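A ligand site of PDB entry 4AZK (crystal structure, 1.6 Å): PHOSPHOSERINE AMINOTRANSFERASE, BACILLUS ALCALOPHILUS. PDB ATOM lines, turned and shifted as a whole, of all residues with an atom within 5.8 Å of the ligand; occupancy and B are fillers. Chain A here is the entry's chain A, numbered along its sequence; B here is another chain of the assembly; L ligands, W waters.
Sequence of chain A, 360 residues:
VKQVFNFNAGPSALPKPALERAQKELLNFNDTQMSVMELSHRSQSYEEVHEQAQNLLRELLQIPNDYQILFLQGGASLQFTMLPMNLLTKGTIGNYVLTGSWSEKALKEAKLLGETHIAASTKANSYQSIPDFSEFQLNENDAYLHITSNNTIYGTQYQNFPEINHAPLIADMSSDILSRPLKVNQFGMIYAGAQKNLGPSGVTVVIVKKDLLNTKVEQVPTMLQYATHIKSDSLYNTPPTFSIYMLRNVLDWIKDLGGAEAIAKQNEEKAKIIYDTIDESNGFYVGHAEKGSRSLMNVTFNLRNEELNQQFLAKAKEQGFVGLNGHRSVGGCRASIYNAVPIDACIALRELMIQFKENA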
ATOM      1  N   ALA A   9     -18.549   6.887   2.695  1.00  0.00           N
ATOM      2  CA  ALA A   9     -17.728   8.032   3.109  1.00  0.00           C
ATOM      3  C   ALA A   9     -16.716   7.732   4.217  1.00  0.00           C
ATOM      4  O   ALA A   9     -15.921   8.601   4.515  1.00  0.00           O
ATOM      5  CB  ALA A   9     -18.632   9.165   3.570  1.00  0.00           C
ATOM      6  N   GLY A  74      -8.357   5.443  18.358  1.00  0.00           N
ATOM      7  CA  GLY A  74      -9.246   6.501  18.811  1.00  0.00           C
ATOM      8  C   GLY A  74      -9.860   7.337  17.708  1.00  0.00           C
ATOM      9  O   GLY A  74     -10.723   8.165  17.969  1.00  0.00           O
ATOM     10  N   GLY A  75      -9.375   7.152  16.485  1.00  0.00           N
ATOM     11  CA  GLY A  75      -9.865   7.898  15.340  1.00  0.00           C
ATOM     12  C   GLY A  75      -9.242   9.273  15.223  1.00  0.00           C
ATOM     13  O   GLY A  75      -8.557   9.747  16.126  1.00  0.00           O
ATOM     14  N   ALA A  76      -9.534   9.986  14.138  1.00  0.00           N
ATOM     15  CA  ALA A  76      -9.195  11.397  14.112  1.00  0.00           C
ATOM     16  C   ALA A  76      -9.861  12.144  15.255  1.00  0.00           C
ATOM     17  O   ALA A  76      -9.322  13.135  15.729  1.00  0.00           O
ATOM     18  CB  ALA A  76      -9.589  12.003  12.753  1.00  0.00           C
ATOM     19  N   SER A  77     -11.046  11.734  15.700  1.00  0.00           N
ATOM     20  CA  SER A  77     -11.717  12.455  16.767  1.00  0.00           C
ATOM     21  C   SER A  77     -10.865  12.519  18.024  1.00  0.00           C
ATOM     22  O   SER A  77     -10.871  13.541  18.703  1.00  0.00           O
ATOM     23  CB  SER A  77     -13.078  11.826  17.089  1.00  0.00           C
ATOM     24  OG  SER A  77     -13.978  11.915  15.998  1.00  0.00           O
ATOM     25  N   LEU A  78     -10.140  11.462  18.369  1.00  0.00           N
ATOM     26  CA  LEU A  78      -9.323  11.558  19.579  1.00  0.00           C
ATOM     27  C   LEU A  78      -8.172  12.559  19.358  1.00  0.00           C
ATOM     28  O   LEU A  78      -7.717  13.203  20.311  1.00  0.00           O
ATOM     29  CB  LEU A  78      -8.800  10.183  19.995  1.00  0.00           C
ATOM     30  CG  LEU A  78      -8.092  10.137  21.381  1.00  0.00           C
ATOM     31  CD1 LEU A  78      -9.014  10.578  22.497  1.00  0.00           C
ATOM     32  CD2 LEU A  78      -7.611   8.787  21.634  1.00  0.00           C
ATOM     33  N   PHE A  80      -8.411  15.322  17.902  1.00  0.00           N
ATOM     34  CA  PHE A  80      -8.958  16.655  18.146  1.00  0.00           C
ATOM     35  C   PHE A  80      -8.610  17.118  19.571  1.00  0.00           C
ATOM     36  O   PHE A  80      -8.411  18.304  19.773  1.00  0.00           O
ATOM     37  CB  PHE A  80     -10.471  16.682  17.980  1.00  0.00           C
ATOM     38  CG  PHE A  80     -10.960  16.455  16.564  1.00  0.00           C
ATOM     39  CD1 PHE A  80     -10.137  16.645  15.471  1.00  0.00           C
ATOM     40  CD2 PHE A  80     -12.274  16.081  16.344  1.00  0.00           C
ATOM     41  CE1 PHE A  80     -10.595  16.442  14.178  1.00  0.00           C
ATOM     42  CE2 PHE A  80     -12.734  15.888  15.048  1.00  0.00           C
ATOM     43  CZ  PHE A  80     -11.903  16.098  13.977  1.00  0.00           C
ATOM     44  N   TRP A 102     -15.875  19.284  10.299  1.00  0.00           N
ATOM     45  CA  TRP A 102     -14.733  18.639  10.940  1.00  0.00           C
ATOM     46  C   TRP A 102     -13.786  19.673  11.535  1.00  0.00           C
ATOM     47  O   TRP A 102     -13.224  19.427  12.579  1.00  0.00           O
ATOM     48  CB  TRP A 102     -14.018  17.679   9.967  1.00  0.00           C
ATOM     49  CG  TRP A 102     -14.877  16.459   9.701  1.00  0.00           C
ATOM     50  CD1 TRP A 102     -15.387  16.051   8.491  1.00  0.00           C
ATOM     51  CD2 TRP A 102     -15.369  15.517  10.675  1.00  0.00           C
ATOM     52  NE1 TRP A 102     -16.143  14.929   8.662  1.00  0.00           N
ATOM     53  CE2 TRP A 102     -16.141  14.579   9.994  1.00  0.00           C
ATOM     54  CE3 TRP A 102     -15.211  15.359  12.059  1.00  0.00           C
ATOM     55  CZ2 TRP A 102     -16.759  13.515  10.629  1.00  0.00           C
ATOM     56  CZ3 TRP A 102     -15.830  14.304  12.691  1.00  0.00           C
ATOM     57  CH2 TRP A 102     -16.587  13.401  11.975  1.00  0.00           C
ATOM     58  N   THR A 148      -8.002  21.784   8.013  1.00  0.00           N
ATOM     59  CA  THR A 148      -8.624  20.536   7.574  1.00  0.00           C
ATOM     60  C   THR A 148      -8.448  20.487   6.075  1.00  0.00           C
ATOM     61  O   THR A 148      -9.051  21.296   5.372  1.00  0.00           O
ATOM     62  CB  THR A 148     -10.129  20.515   7.937  1.00  0.00           C
ATOM     63  OG1 THR A 148     -10.312  20.881   9.331  1.00  0.00           O
ATOM     64  CG2 THR A 148     -10.722  19.130   7.717  1.00  0.00           C
ATOM     65  N   ASN A 150      -9.205  18.409   3.642  1.00  0.00           N
ATOM     66  CA  ASN A 150     -10.370  18.007   2.840  1.00  0.00           C
ATOM     67  C   ASN A 150     -11.574  17.999   3.770  1.00  0.00           C
ATOM     68  O   ASN A 150     -11.588  17.317   4.812  1.00  0.00           O
ATOM     69  CB  ASN A 150     -10.127  16.682   2.159  1.00  0.00           C
ATOM     70  CG  ASN A 150     -11.228  16.326   1.172  1.00  0.00           C
ATOM     71  OD1 ASN A 150     -11.232  16.816   0.043  1.00  0.00           O
ATOM     72  ND2 ASN A 150     -12.160  15.498   1.583  1.00  0.00           N
ATOM     73  N   ASN A 151     -12.598  18.773   3.428  1.00  0.00           N
ATOM     74  CA  ASN A 151     -13.731  18.972   4.307  1.00  0.00           C
ATOM     75  C   ASN A 151     -14.821  18.018   3.862  1.00  0.00           C
ATOM     76  O   ASN A 151     -15.631  18.292   2.963  1.00  0.00           O
ATOM     77  CB  ASN A 151     -14.158  20.438   4.246  1.00  0.00           C
ATOM     78  CG  ASN A 151     -13.022  21.345   4.588  1.00  0.00           C
ATOM     79  OD1 ASN A 151     -12.645  21.429   5.757  1.00  0.00           O
ATOM     80  ND2 ASN A 151     -12.437  21.974   3.589  1.00  0.00           N
ATOM     81  N   THR A 152     -14.778  16.851   4.470  1.00  0.00           N
ATOM     82  CA  THR A 152     -15.504  15.657   4.024  1.00  0.00           C
ATOM     83  C   THR A 152     -16.993  15.862   3.836  1.00  0.00           C
ATOM     84  O   THR A 152     -17.584  15.291   2.912  1.00  0.00           O
ATOM     85  CB  THR A 152     -15.250  14.549   5.029  1.00  0.00           C
ATOM     86  OG1 THR A 152     -13.893  14.692   5.499  1.00  0.00           O
ATOM     87  CG2 THR A 152     -15.432  13.192   4.365  1.00  0.00           C
ATOM     88  N   ASP A 172      -5.650  18.056   9.787  1.00  0.00           N
ATOM     89  CA  ASP A 172      -6.521  16.875   9.711  1.00  0.00           C
ATOM     90  C   ASP A 172      -6.694  16.516   8.221  1.00  0.00           C
ATOM     91  O   ASP A 172      -7.418  17.210   7.487  1.00  0.00           O
ATOM     92  CB  ASP A 172      -7.879  17.225  10.316  1.00  0.00           C
ATOM     93  CG  ASP A 172      -8.874  16.087  10.237  1.00  0.00           C
ATOM     94  OD1 ASP A 172      -8.567  15.017   9.650  1.00  0.00           O
ATOM     95  OD2 ASP A 172     -10.005  16.304  10.747  1.00  0.00           O
ATOM     96  N   MET A 173      -5.977  15.503   7.798  1.00  0.00           N
ATOM     97  CA  MET A 173      -5.967  15.053   6.396  1.00  0.00           C
ATOM     98  C   MET A 173      -6.723  13.731   6.252  1.00  0.00           C
ATOM     99  O   MET A 173      -6.477  12.990   5.303  1.00  0.00           O
ATOM    100  CB  MET A 173      -4.521  14.935   5.868  1.00  0.00           C
ATOM    101  CG  MET A 173      -3.783  16.243   5.847  1.00  0.00           C
ATOM    102  SD  MET A 173      -2.288  16.109   4.890  1.00  0.00           S
ATOM    103  CE  MET A 173      -1.750  17.827   4.920  1.00  0.00           C
ATOM    104  N   SER A 174      -7.668  13.449   7.161  1.00  0.00           N
ATOM    105  CA  SER A 174      -8.361  12.164   7.164  1.00  0.00           C
ATOM    106  C   SER A 174      -8.888  11.775   5.792  1.00  0.00           C
ATOM    107  O   SER A 174      -8.741  10.644   5.393  1.00  0.00           O
ATOM    108  CB  SER A 174      -9.532  12.166   8.141  1.00  0.00           C
ATOM    109  OG  SER A 174      -9.099  12.316   9.480  1.00  0.00           O
ATOM    110  N   SER A 175      -9.534  12.700   5.108  1.00  0.00           N
ATOM    111  CA  SER A 175     -10.227  12.305   3.897  1.00  0.00           C
ATOM    112  C   SER A 175      -9.491  12.568   2.583  1.00  0.00           C
ATOM    113  O   SER A 175     -10.058  12.304   1.515  1.00  0.00           O
ATOM    114  CB  SER A 175     -11.635  12.880   3.919  1.00  0.00           C
ATOM    115  OG  SER A 175     -11.603  14.301   4.140  1.00  0.00           O
ATOM    116  N   GLY A 193      -7.544   9.485  10.331  1.00  0.00           N
ATOM    117  CA  GLY A 193      -8.150   8.172  10.498  1.00  0.00           C
ATOM    118  C   GLY A 193      -7.888   7.370   9.229  1.00  0.00           C
ATOM    119  O   GLY A 193      -7.963   7.893   8.137  1.00  0.00           O
ATOM    120  N   GLN A 195      -9.548   5.043   7.716  1.00  0.00           N
ATOM    121  CA  GLN A 195     -10.690   4.446   7.054  1.00  0.00           C
ATOM    122  C   GLN A 195     -11.274   5.193   5.862  1.00  0.00           C
ATOM    123  O   GLN A 195     -12.287   4.761   5.314  1.00  0.00           O
ATOM    124  CB  GLN A 195     -11.786   4.193   8.063  1.00  0.00           C
ATOM    125  CG  GLN A 195     -12.448   5.416   8.609  1.00  0.00           C
ATOM    126  CD  GLN A 195     -11.787   5.987   9.852  1.00  0.00           C
ATOM    127  OE1 GLN A 195     -10.680   5.617  10.214  1.00  0.00           O
ATOM    128  NE2 GLN A 195     -12.471   6.928  10.492  1.00  0.00           N
ATOM    129  N   LYS A 196     -10.681   6.303   5.443  1.00  0.00           N
ATOM    130  CA  LYS A 196     -11.164   6.925   4.207  1.00  0.00           C
ATOM    131  C   LYS A 196     -10.249   6.541   3.039  1.00  0.00           C
ATOM    132  O   LYS A 196     -10.705   5.982   2.053  1.00  0.00           O
ATOM    133  CB  LYS A 196     -11.387   8.454   4.367  1.00  0.00           C
ATOM    134  CG  LYS A 196     -11.542   8.983   5.791  1.00  0.00           C
ATOM    135  CD  LYS A 196     -12.933   9.429   6.219  1.00  0.00           C
ATOM    136  CE  LYS A 196     -12.966   9.896   7.719  1.00  0.00           C
ATOM    137  NZ  LYS A 196     -14.236  10.611   8.094  1.00  0.00           N
ATOM    138  N   THR A 204      -5.379   5.251  13.383  1.00  0.00           N
ATOM    139  CA  THR A 204      -5.175   6.630  13.003  1.00  0.00           C
ATOM    140  C   THR A 204      -3.686   6.827  12.793  1.00  0.00           C
ATOM    141  O   THR A 204      -2.874   6.447  13.629  1.00  0.00           O
ATOM    142  CB  THR A 204      -5.723   7.530  14.130  1.00  0.00           C
ATOM    143  OG1 THR A 204      -7.098   7.198  14.326  1.00  0.00           O
ATOM    144  CG2 THR A 204      -5.601   8.997  13.802  1.00  0.00           C
ATOM    145  N   TYR A 338     -12.707   8.170  -2.886  1.00  0.00           N
ATOM    146  CA  TYR A 338     -11.384   7.926  -2.347  1.00  0.00           C
ATOM    147  C   TYR A 338     -10.553   7.034  -3.270  1.00  0.00           C
ATOM    148  O   TYR A 338     -11.085   6.452  -4.219  1.00  0.00           O
ATOM    149  CB  TYR A 338     -11.523   7.245  -0.979  1.00  0.00           C
ATOM    150  CG  TYR A 338     -12.329   8.034   0.038  1.00  0.00           C
ATOM    151  CD1 TYR A 338     -12.035   9.358   0.320  1.00  0.00           C
ATOM    152  CD2 TYR A 338     -13.400   7.454   0.685  1.00  0.00           C
ATOM    153  CE1 TYR A 338     -12.790  10.062   1.247  1.00  0.00           C
ATOM    154  CE2 TYR A 338     -14.125   8.147   1.629  1.00  0.00           C
ATOM    155  CZ  TYR A 338     -13.815   9.452   1.912  1.00  0.00           C
ATOM    156  OH  TYR A 338     -14.550  10.178   2.832  1.00  0.00           O
ATOM    157  N   GLN B  73     -12.342   2.336  21.491  1.00  0.00           N
ATOM    158  CA  GLN B  73     -10.942   2.165  21.113  1.00  0.00           C
ATOM    159  C   GLN B  73     -10.036   2.566  22.268  1.00  0.00           C
ATOM    160  O   GLN B  73     -10.463   3.261  23.198  1.00  0.00           O
ATOM    161  CB  GLN B  73     -10.647   3.008  19.873  1.00  0.00           C
ATOM    162  CG  GLN B  73     -11.467   2.641  18.649  1.00  0.00           C
ATOM    163  CD  GLN B  73     -11.035   3.466  17.445  1.00  0.00           C
ATOM    164  OE1 GLN B  73      -9.873   3.392  17.029  1.00  0.00           O
ATOM    165  NE2 GLN B  73     -11.919   4.295  16.942  1.00  0.00           N
ATOM    166  N   ASN B 237     -18.099   8.294  16.990  1.00  0.00           N
ATOM    167  CA  ASN B 237     -17.216   8.360  15.844  1.00  0.00           C
ATOM    168  C   ASN B 237     -17.100   6.995  15.202  1.00  0.00           C
ATOM    169  O   ASN B 237     -17.852   6.077  15.541  1.00  0.00           O
ATOM    170  CB  ASN B 237     -15.853   8.987  16.196  1.00  0.00           C
ATOM    171  CG  ASN B 237     -14.968   8.058  17.010  1.00  0.00           C
ATOM    172  OD1 ASN B 237     -15.466   7.229  17.782  1.00  0.00           O
ATOM    173  ND2 ASN B 237     -13.660   8.166  16.814  1.00  0.00           N
ATOM    174  N   THR B 238     -16.168   6.821  14.275  1.00  0.00           N
ATOM    175  CA  THR B 238     -16.121   5.570  13.526  1.00  0.00           C
ATOM    176  C   THR B 238     -15.588   4.439  14.389  1.00  0.00           C
ATOM    177  O   THR B 238     -14.483   4.542  14.927  1.00  0.00           O
ATOM    178  CB  THR B 238     -15.265   5.698  12.293  1.00  0.00           C
ATOM    179  OG1 THR B 238     -15.645   6.846  11.536  1.00  0.00           O
ATOM    180  CG2 THR B 238     -15.440   4.481  11.404  1.00  0.00           C
HETATM  181  N1  LIG L   1     -11.916  14.484  10.252  1.00  0.00           N
HETATM  182  C1  LIG L   1     -12.308  14.251   8.931  1.00  0.00           C
HETATM  183  C2  LIG L   1     -11.836  15.249   7.910  1.00  0.00           C
HETATM  184  C3  LIG L   1     -13.110  13.172   8.612  1.00  0.00           C
HETATM  185  O1  LIG L   1     -13.442  13.012   7.417  1.00  0.00           O
HETATM  186  C4  LIG L   1     -13.492  12.269   9.620  1.00  0.00           C
HETATM  187  C5  LIG L   1     -14.356  11.052   9.363  1.00  0.00           C
HETATM  188  C6  LIG L   1     -13.116  12.521  10.940  1.00  0.00           C
HETATM  189  C7  LIG L   1     -12.316  13.602  11.234  1.00  0.00           C
HETATM  190  C8  LIG L   1     -13.526  11.612  12.072  1.00  0.00           C
HETATM  191  O2  LIG L   1     -12.786  10.387  12.124  1.00  0.00           O
HETATM  192  P1  LIG L   1     -13.103   9.264  13.241  1.00  0.00           P
HETATM  193  O3  LIG L   1     -14.495   8.817  12.967  1.00  0.00           O
HETATM  194  O4  LIG L   1     -12.934   9.957  14.578  1.00  0.00           O
HETATM  195  O5  LIG L   1     -12.055   8.301  12.933  1.00  0.00           O
HETATM  196  O   HOH W   1     -12.205   5.911  14.323  1.00  0.00           O
HETATM  197  O   HOH W   2     -10.657  10.012  10.248  1.00  0.00           O
HETATM  198  O   HOH W   3     -16.943  10.077  12.834  1.00  0.00           O
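NZ of Lys 196 is covalently linked to C5 of the ligand (1.3 Å).
The side-chain amide nitrogen of Asn 237 of chain B is in hydrogen-bond range of an oxygen (O4) of the ligand (3.0 Å).
O4 of the ligand lies within hydrogen-bond range of N of Ser 77 (2.8 Å).
The side-chain hydroxyl of Thr 238 of chain B is in hydrogen-bond range of an oxygen (O3) of the ligand (2.7 Å).
An oxygen (O1) of the ligand lies within hydrogen-bond range of the side-chain hydroxyl (OG1) of Thr 152 (2.6 Å).
The backbone NH (N) of Thr 238 of chain B lies within hydrogen-bond range of an oxygen (O3) of the ligand (2.9 Å).
NE2 of Gln 195 sits at hydrogen-bond distance from O5 of the ligand (2.8 Å).
N of Ala 76 is in hydrogen-bond range of O5 of the ligand, at 3.3 Å.
O4 of the ligand sits at hydrogen-bond distance from OG of Ser 77, 2.6 Å away.
The side-chain carboxylate of Asp 172 is in hydrogen-bond range of a nitrogen (N1) of the ligand, 2.7 Å away.
The side-chain hydroxyl (OG1) of Thr 152 sits at hydrogen-bond distance from the side-chain hydroxyl (OG) of Ser 175 (2.7 Å).
The side-chain amide nitrogen (ND2) of Asn 150 lies within hydrogen-bond range of the side-chain hydroxyl (OG) of Ser 175.
The backbone carbonyl oxygen (O) of Gly 74 is in hydrogen-bond range of the side-chain amide nitrogen (ND2) of Asn 237 of chain B (3.2 Å).
The side-chain hydroxyl of Thr 238 of chain B lies within hydrogen-bond range of the side-chain amide nitrogen of Gln 195 (3.3 Å).
N of Gly 75 lies close to OG1 of Thr 204 (3.1 Å).
OG of Ser 174 is in hydrogen-bond range of OD1 of Asp 172, 2.8 Å away.
NE2 of Gln 73 of chain B lies within hydrogen-bond range of O of Thr 238 of chain B.
The backbone NH (N) of Gly 193 lies within hydrogen-bond range of the side-chain hydroxyl (OG) of Ser 174 (3.3 Å).
Gly 75 touches the ligand.
CZ of Phe 80 touches C7 of the ligand, 3.7 Å away.
CG of Trp 102 touches C1 of the ligand (3.5 Å).
Asn 150 touches the ligand (O to C2, 3.7 Å).
CB of Ser 174 touches C1 of the ligand, 3.6 Å away.
Ser 175 touches the ligand (OG to C2, 3.9 Å).
Hydrophobic or aromatic side chains that line the ligand: Ala 76, Phe 80 and Trp 102.
14 residues have an atom within 4 Å of the ligand: Gly 75, Ala 76, Ser 77, Phe 80, Trp 102, Asn 150, Thr 152, Asp 172, Ser 174, Ser 175, Gln 195, Lys 196, Asn 237 of chain B and Thr 238 of chain B.
Water W1 lies within hydrogen-bond range of the backbone carbonyl oxygen (O) of Thr 238 of chain B (2.7 Å), an oxygen (O5) of the ligand (2.8 Å) and the side-chain amide nitrogen (NE2) of Gln 73 of chain B (3.1 Å).
Water W2 lies within hydrogen-bond range of an oxygen (O2) of the ligand (2.9 Å), the side-chain hydroxyl (OG) of Ser 174 (2.9 Å) and the backbone NH (N) of Gly 193 (3.2 Å).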
